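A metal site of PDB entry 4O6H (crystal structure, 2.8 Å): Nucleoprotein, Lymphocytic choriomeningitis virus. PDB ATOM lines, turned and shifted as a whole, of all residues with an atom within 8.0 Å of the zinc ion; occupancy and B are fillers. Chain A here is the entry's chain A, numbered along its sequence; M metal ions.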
ATOM      1  N   GLU A  59      23.690 -21.144 -25.592  1.00  0.00           N
ATOM      2  CA  GLU A  59      24.135 -22.194 -26.492  1.00  0.00           C
ATOM      3  C   GLU A  59      24.130 -21.599 -27.896  1.00  0.00           C
ATOM      4  O   GLU A  59      23.316 -20.734 -28.209  1.00  0.00           O
ATOM      5  CB  GLU A  59      23.240 -23.426 -26.404  1.00  0.00           C
ATOM      6  CG  GLU A  59      23.263 -24.099 -25.030  1.00  0.00           C
ATOM      7  CD  GLU A  59      24.651 -24.584 -24.631  1.00  0.00           C
ATOM      8  OE1 GLU A  59      25.421 -24.989 -25.535  1.00  0.00           O
ATOM      9  OE2 GLU A  59      24.970 -24.555 -23.431  1.00  0.00           O
ATOM     10  N   VAL A  66      21.204 -19.832 -29.959  1.00  0.00           N
ATOM     11  CA  VAL A  66      20.057 -20.702 -30.199  1.00  0.00           C
ATOM     12  C   VAL A  66      19.280 -20.937 -28.905  1.00  0.00           C
ATOM     13  O   VAL A  66      18.091 -21.259 -28.939  1.00  0.00           O
ATOM     14  CB  VAL A  66      20.484 -22.059 -30.783  1.00  0.00           C
ATOM     15  CG1 VAL A  66      20.790 -21.924 -32.260  1.00  0.00           C
ATOM     16  CG2 VAL A  66      21.688 -22.606 -30.040  1.00  0.00           C
ATOM     17  N   GLU A  67      19.954 -20.792 -27.774  1.00  0.00           N
ATOM     18  CA  GLU A  67      19.309 -20.913 -26.473  1.00  0.00           C
ATOM     19  C   GLU A  67      19.940 -19.952 -25.477  1.00  0.00           C
ATOM     20  O   GLU A  67      21.154 -19.949 -25.301  1.00  0.00           O
ATOM     21  CB  GLU A  67      19.411 -22.339 -25.958  1.00  0.00           C
ATOM     22  CG  GLU A  67      18.516 -22.625 -24.765  1.00  0.00           C
ATOM     23  CD  GLU A  67      18.723 -24.002 -24.177  1.00  0.00           C
ATOM     24  OE1 GLU A  67      19.839 -24.542 -24.313  1.00  0.00           O
ATOM     25  OE2 GLU A  67      17.769 -24.538 -23.580  1.00  0.00           O
ATOM     26  N   ILE A  68      19.108 -19.131 -24.843  1.00  0.00           N
ATOM     27  CA  ILE A  68      19.570 -18.164 -23.856  1.00  0.00           C
ATOM     28  C   ILE A  68      18.934 -18.464 -22.509  1.00  0.00           C
ATOM     29  O   ILE A  68      17.741 -18.757 -22.421  1.00  0.00           O
ATOM     30  CB  ILE A  68      19.235 -16.703 -24.264  1.00  0.00           C
ATOM     31  CG1 ILE A  68      19.960 -16.331 -25.553  1.00  0.00           C
ATOM     32  CG2 ILE A  68      19.625 -15.721 -23.163  1.00  0.00           C
ATOM     33  CD1 ILE A  68      19.229 -16.725 -26.825  1.00  0.00           C
ATOM     34  N   ALA A  69      19.749 -18.384 -21.460  1.00  0.00           N
ATOM     35  CA  ALA A  69      19.259 -18.559 -20.093  1.00  0.00           C
ATOM     36  C   ALA A  69      19.852 -17.492 -19.194  1.00  0.00           C
ATOM     37  O   ALA A  69      21.055 -17.228 -19.230  1.00  0.00           O
ATOM     38  CB  ALA A  69      19.610 -19.940 -19.577  1.00  0.00           C
ATOM     39  N   HIS A  80      14.353 -17.981 -19.828  1.00  0.00           N
ATOM     40  CA  HIS A  80      14.788 -19.063 -20.701  1.00  0.00           C
ATOM     41  C   HIS A  80      13.991 -19.047 -21.994  1.00  0.00           C
ATOM     42  O   HIS A  80      12.767 -19.166 -21.977  1.00  0.00           O
ATOM     43  CB  HIS A  80      14.640 -20.404 -19.992  1.00  0.00           C
ATOM     44  CG  HIS A  80      15.089 -21.580 -20.810  1.00  0.00           C
ATOM     45  ND1 HIS A  80      14.477 -22.806 -20.760  1.00  0.00           N
ATOM     46  CD2 HIS A  80      16.106 -21.705 -21.695  1.00  0.00           C
ATOM     47  CE1 HIS A  80      15.079 -23.644 -21.589  1.00  0.00           C
ATOM     48  NE2 HIS A  80      16.081 -22.997 -22.165  1.00  0.00           N
ATOM     49  N   PHE A  81      14.686 -18.912 -23.115  1.00  0.00           N
ATOM     50  CA  PHE A  81      14.035 -18.893 -24.417  1.00  0.00           C
ATOM     51  C   PHE A  81      14.990 -19.355 -25.507  1.00  0.00           C
ATOM     52  O   PHE A  81      16.149 -19.666 -25.235  1.00  0.00           O
ATOM     53  CB  PHE A  81      13.520 -17.487 -24.729  1.00  0.00           C
ATOM     54  CG  PHE A  81      14.585 -16.433 -24.773  1.00  0.00           C
ATOM     55  CD1 PHE A  81      15.077 -15.856 -23.617  1.00  0.00           C
ATOM     56  CD2 PHE A  81      15.098 -16.002 -25.992  1.00  0.00           C
ATOM     57  CE1 PHE A  81      16.056 -14.880 -23.661  1.00  0.00           C
ATOM     58  CE2 PHE A  81      16.074 -15.028 -26.045  1.00  0.00           C
ATOM     59  CZ  PHE A  81      16.554 -14.468 -24.879  1.00  0.00           C
ATOM     60  N   TYR A  82      14.490 -19.403 -26.737  1.00  0.00           N
ATOM     61  CA  TYR A  82      15.233 -19.978 -27.855  1.00  0.00           C
ATOM     62  C   TYR A  82      15.284 -19.043 -29.066  1.00  0.00           C
ATOM     63  O   TYR A  82      14.634 -17.997 -29.085  1.00  0.00           O
ATOM     64  CB  TYR A  82      14.608 -21.312 -28.249  1.00  0.00           C
ATOM     65  CG  TYR A  82      14.181 -22.145 -27.062  1.00  0.00           C
ATOM     66  CD1 TYR A  82      15.106 -22.882 -26.330  1.00  0.00           C
ATOM     67  CD2 TYR A  82      12.857 -22.172 -26.663  1.00  0.00           C
ATOM     68  CE1 TYR A  82      14.717 -23.629 -25.244  1.00  0.00           C
ATOM     69  CE2 TYR A  82      12.448 -22.929 -25.578  1.00  0.00           C
ATOM     70  CZ  TYR A  82      13.392 -23.651 -24.869  1.00  0.00           C
ATOM     71  OH  TYR A  82      12.992 -24.405 -23.787  1.00  0.00           O
ATOM     72  N   HIS A  99      25.083 -29.058 -27.684  1.00  0.00           N
ATOM     73  CA  HIS A  99      23.753 -28.913 -27.095  1.00  0.00           C
ATOM     74  C   HIS A  99      22.739 -29.957 -27.560  1.00  0.00           C
ATOM     75  O   HIS A  99      21.716 -30.148 -26.915  1.00  0.00           O
ATOM     76  CB  HIS A  99      23.205 -27.510 -27.353  1.00  0.00           C
ATOM     77  CG  HIS A  99      23.293 -27.059 -28.782  1.00  0.00           C
ATOM     78  ND1 HIS A  99      22.566 -27.649 -29.798  1.00  0.00           N
ATOM     79  CD2 HIS A  99      23.991 -26.062 -29.366  1.00  0.00           C
ATOM     80  CE1 HIS A  99      22.827 -27.048 -30.935  1.00  0.00           C
ATOM     81  NE2 HIS A  99      23.699 -26.078 -30.701  1.00  0.00           N
ATOM     82  N   MET A 101      20.559 -30.056 -29.906  1.00  0.00           N
ATOM     83  CA  MET A 101      19.228 -29.499 -30.138  1.00  0.00           C
ATOM     84  C   MET A 101      18.753 -29.753 -31.549  1.00  0.00           C
ATOM     85  O   MET A 101      19.563 -29.845 -32.478  1.00  0.00           O
ATOM     86  CB  MET A 101      19.217 -27.997 -29.853  1.00  0.00           C
ATOM     87  CG  MET A 101      19.157 -27.664 -28.376  1.00  0.00           C
ATOM     88  SD  MET A 101      18.829 -25.926 -28.073  1.00  0.00           S
ATOM     89  CE  MET A 101      20.446 -25.238 -28.350  1.00  0.00           C
ATOM     90  N   TRP A 167      20.321 -32.127 -13.719  1.00  0.00           N
ATOM     91  CA  TRP A 167      19.467 -32.634 -14.789  1.00  0.00           C
ATOM     92  C   TRP A 167      18.305 -33.473 -14.247  1.00  0.00           C
ATOM     93  O   TRP A 167      17.230 -33.521 -14.834  1.00  0.00           O
ATOM     94  CB  TRP A 167      20.268 -33.481 -15.782  1.00  0.00           C
ATOM     95  CG  TRP A 167      20.894 -32.691 -16.898  1.00  0.00           C
ATOM     96  CD1 TRP A 167      22.203 -32.336 -17.011  1.00  0.00           C
ATOM     97  CD2 TRP A 167      20.230 -32.184 -18.057  1.00  0.00           C
ATOM     98  NE1 TRP A 167      22.399 -31.625 -18.173  1.00  0.00           N
ATOM     99  CE2 TRP A 167      21.208 -31.520 -18.833  1.00  0.00           C
ATOM    100  CE3 TRP A 167      18.915 -32.217 -18.515  1.00  0.00           C
ATOM    101  CZ2 TRP A 167      20.899 -30.902 -20.037  1.00  0.00           C
ATOM    102  CZ3 TRP A 167      18.611 -31.608 -19.717  1.00  0.00           C
ATOM    103  CH2 TRP A 167      19.596 -30.955 -20.458  1.00  0.00           C
ATOM    104  N   GLY A 171      15.649 -31.061 -14.939  1.00  0.00           N
ATOM    105  CA  GLY A 171      15.672 -31.409 -16.355  1.00  0.00           C
ATOM    106  C   GLY A 171      14.341 -31.187 -17.044  1.00  0.00           C
ATOM    107  O   GLY A 171      14.284 -31.020 -18.263  1.00  0.00           O
ATOM    108  N   LEU A 173      12.616 -28.695 -17.054  1.00  0.00           N
ATOM    109  CA  LEU A 173      12.495 -27.303 -17.484  1.00  0.00           C
ATOM    110  C   LEU A 173      12.808 -27.131 -18.966  1.00  0.00           C
ATOM    111  O   LEU A 173      12.252 -26.248 -19.626  1.00  0.00           O
ATOM    112  CB  LEU A 173      13.406 -26.401 -16.644  1.00  0.00           C
ATOM    113  CG  LEU A 173      13.086 -26.309 -15.153  1.00  0.00           C
ATOM    114  CD1 LEU A 173      14.153 -25.517 -14.425  1.00  0.00           C
ATOM    115  CD2 LEU A 173      11.721 -25.690 -14.933  1.00  0.00           C
ATOM    116  N   CYS A 174      13.702 -27.970 -19.477  1.00  0.00           N
ATOM    117  CA  CYS A 174      14.085 -27.915 -20.877  1.00  0.00           C
ATOM    118  C   CYS A 174      14.206 -29.315 -21.479  1.00  0.00           C
ATOM    119  O   CYS A 174      15.030 -30.120 -21.037  1.00  0.00           O
ATOM    120  CB  CYS A 174      15.413 -27.174 -21.049  1.00  0.00           C
ATOM    121  SG  CYS A 174      15.892 -26.920 -22.767  1.00  0.00           S
ATOM    122  N   LYS A 175      13.367 -29.588 -22.467  1.00  0.00           N
ATOM    123  CA  LYS A 175      13.357 -30.871 -23.157  1.00  0.00           C
ATOM    124  C   LYS A 175      13.677 -30.683 -24.636  1.00  0.00           C
ATOM    125  O   LYS A 175      13.114 -31.348 -25.503  1.00  0.00           O
ATOM    126  CB  LYS A 175      11.996 -31.559 -22.985  1.00  0.00           C
ATOM    127  CG  LYS A 175      11.709 -31.958 -21.542  1.00  0.00           C
ATOM    128  CD  LYS A 175      10.385 -32.710 -21.423  1.00  0.00           C
ATOM    129  CE  LYS A 175       9.194 -31.795 -21.649  1.00  0.00           C
ATOM    130  NZ  LYS A 175       9.145 -30.693 -20.648  1.00  0.00           N
ATOM    131  N   MET A 176      14.590 -29.763 -24.906  1.00  0.00           N
ATOM    132  CA  MET A 176      14.961 -29.407 -26.277  1.00  0.00           C
ATOM    133  C   MET A 176      16.171 -30.201 -26.740  1.00  0.00           C
ATOM    134  O   MET A 176      16.390 -30.361 -27.941  1.00  0.00           O
ATOM    135  CB  MET A 176      15.254 -27.915 -26.364  1.00  0.00           C
ATOM    136  CG  MET A 176      14.073 -27.039 -25.998  1.00  0.00           C
ATOM    137  SD  MET A 176      12.838 -26.927 -27.305  1.00  0.00           S
ATOM    138  CE  MET A 176      13.736 -25.983 -28.537  1.00  0.00           C
ATOM    139  N   HIS A 177      16.956 -30.689 -25.790  1.00  0.00           N
ATOM    140  CA  HIS A 177      18.206 -31.377 -26.095  1.00  0.00           C
ATOM    141  C   HIS A 177      17.985 -32.874 -26.216  1.00  0.00           C
ATOM    142  O   HIS A 177      18.371 -33.653 -25.348  1.00  0.00           O
ATOM    143  CB  HIS A 177      19.231 -31.055 -25.012  1.00  0.00           C
ATOM    144  CG  HIS A 177      19.346 -29.602 -24.721  1.00  0.00           C
ATOM    145  ND1 HIS A 177      20.129 -28.744 -25.474  1.00  0.00           N
ATOM    146  CD2 HIS A 177      18.764 -28.828 -23.772  1.00  0.00           C
ATOM    147  CE1 HIS A 177      20.028 -27.523 -24.985  1.00  0.00           C
ATOM    148  NE2 HIS A 177      19.202 -27.552 -23.959  1.00  0.00           N
ATOM    149  N   PRO A 191      24.100 -33.620 -22.806  1.00  0.00           N
ATOM    150  CA  PRO A 191      24.076 -32.390 -23.611  1.00  0.00           C
ATOM    151  C   PRO A 191      24.153 -31.124 -22.757  1.00  0.00           C
ATOM    152  O   PRO A 191      23.814 -31.177 -21.570  1.00  0.00           O
ATOM    153  CB  PRO A 191      22.734 -32.462 -24.348  1.00  0.00           C
ATOM    154  CG  PRO A 191      22.188 -33.832 -24.093  1.00  0.00           C
ATOM    155  CD  PRO A 191      22.792 -34.280 -22.806  1.00  0.00           C
ATOM    156  N   HIS A 192      24.585 -30.023 -23.351  1.00  0.00           N
ATOM    157  CA  HIS A 192      24.670 -28.753 -22.633  1.00  0.00           C
ATOM    158  C   HIS A 192      23.421 -27.910 -22.847  1.00  0.00           C
ATOM    159  O   HIS A 192      23.045 -27.607 -23.984  1.00  0.00           O
ATOM    160  CB  HIS A 192      25.905 -27.969 -23.085  1.00  0.00           C
ATOM    161  CG  HIS A 192      27.185 -28.502 -22.525  1.00  0.00           C
ATOM    162  ND1 HIS A 192      28.402 -28.347 -23.156  1.00  0.00           N
ATOM    163  CD2 HIS A 192      27.445 -29.183 -21.382  1.00  0.00           C
ATOM    164  CE1 HIS A 192      29.346 -28.905 -22.435  1.00  0.00           C
ATOM    165  NE2 HIS A 192      28.805 -29.419 -21.353  1.00  0.00           N
ATOM    166  N   CYS A 193      22.776 -27.541 -21.741  1.00  0.00           N
ATOM    167  CA  CYS A 193      21.606 -26.670 -21.777  1.00  0.00           C
ATOM    168  C   CYS A 193      21.942 -25.327 -21.137  1.00  0.00           C
ATOM    169  O   CYS A 193      22.547 -25.277 -20.061  1.00  0.00           O
ATOM    170  CB  CYS A 193      20.435 -27.325 -21.038  1.00  0.00           C
ATOM    171  SG  CYS A 193      18.989 -26.251 -20.809  1.00  0.00           S
ATOM    172  N   ALA A 194      21.542 -24.250 -21.797  1.00  0.00           N
ATOM    173  CA  ALA A 194      21.794 -22.903 -21.291  1.00  0.00           C
ATOM    174  C   ALA A 194      21.247 -22.762 -19.878  1.00  0.00           C
ATOM    175  O   ALA A 194      21.893 -22.171 -19.017  1.00  0.00           O
ATOM    176  CB  ALA A 194      21.178 -21.862 -22.209  1.00  0.00           C
ATOM    177  N   LEU A 195      20.077 -23.324 -19.633  1.00  0.00           N
ATOM    178  CA  LEU A 195      19.423 -23.207 -18.325  1.00  0.00           C
ATOM    179  C   LEU A 195      20.075 -24.120 -17.290  1.00  0.00           C
ATOM    180  O   LEU A 195      20.316 -23.699 -16.157  1.00  0.00           O
ATOM    181  CB  LEU A 195      17.940 -23.526 -18.443  1.00  0.00           C
ATOM    182  CG  LEU A 195      17.126 -23.400 -17.148  1.00  0.00           C
ATOM    183  CD1 LEU A 195      17.193 -21.996 -16.590  1.00  0.00           C
ATOM    184  CD2 LEU A 195      15.683 -23.805 -17.412  1.00  0.00           C
ATOM    185  N   MET A 196      20.348 -25.366 -17.674  1.00  0.00           N
ATOM    186  CA  MET A 196      20.988 -26.306 -16.770  1.00  0.00           C
ATOM    187  C   MET A 196      22.398 -25.840 -16.422  1.00  0.00           C
ATOM    188  O   MET A 196      22.846 -25.968 -15.284  1.00  0.00           O
ATOM    189  CB  MET A 196      21.033 -27.703 -17.385  1.00  0.00           C
ATOM    190  CG  MET A 196      19.673 -28.280 -17.770  1.00  0.00           C
ATOM    191  SD  MET A 196      18.584 -28.562 -16.357  1.00  0.00           S
ATOM    192  CE  MET A 196      17.696 -27.017 -16.284  1.00  0.00           C
ATOM    193  N   ASP A 197      23.093 -25.294 -17.415  1.00  0.00           N
ATOM    194  CA  ASP A 197      24.428 -24.762 -17.205  1.00  0.00           C
ATOM    195  C   ASP A 197      24.421 -23.751 -16.058  1.00  0.00           C
ATOM    196  O   ASP A 197      25.255 -23.824 -15.153  1.00  0.00           O
ATOM    197  CB  ASP A 197      24.971 -24.111 -18.476  1.00  0.00           C
ATOM    198  CG  ASP A 197      25.675 -25.103 -19.395  1.00  0.00           C
ATOM    199  OD1 ASP A 197      25.547 -26.329 -19.172  1.00  0.00           O
ATOM    200  OD2 ASP A 197      26.359 -24.640 -20.330  1.00  0.00           O
HETATM  201 ZN    ZN M   1      17.952 -26.269 -22.755  1.00  0.00          ZN
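Residues that only touch the zinc ion: His 80.
Of the 24 residues printed, 5 come within 4 Å of the zinc ion.
The nearest printed residue that does not touch the zinc ion is Ala 194 (4.2 Å).
OE2 of Glu 67 binds the zinc ion (1.9 Å).
The zinc ion is bound by NE2 of His 177, 2.2 Å away.
The zinc ion is bound by the side-chain sulfur (SG) of Cys 174 (2.2 Å).
The zinc ion is bound by SG of Cys 193.
OE2 of Glu 67 sits close to NE2 of His 80, at 2.7 Å.
The backbone NH (N) of Ala 194 lies within hydrogen-bond range of the side-chain carboxylate (OE1) of Glu 67 (3.1 Å).
N of Glu 59 is in hydrogen-bond range of O of Glu 67, at 2.8 Å.
ND1 of His 177 sits close to O of His 192, 3.5 Å away.
ND1 of His 177 is in hydrogen-bond range of O of His 99.
The backbone NH of Met 176 lies close to the side-chain sulfur of Cys 174, at 3.8 Å.
SG of Cys 193 lies close to N of Leu 195, 3.3 Å away.
The side-chain sulfur of Cys 193 sits close to the backbone NH of Met 196 (3.5 Å).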
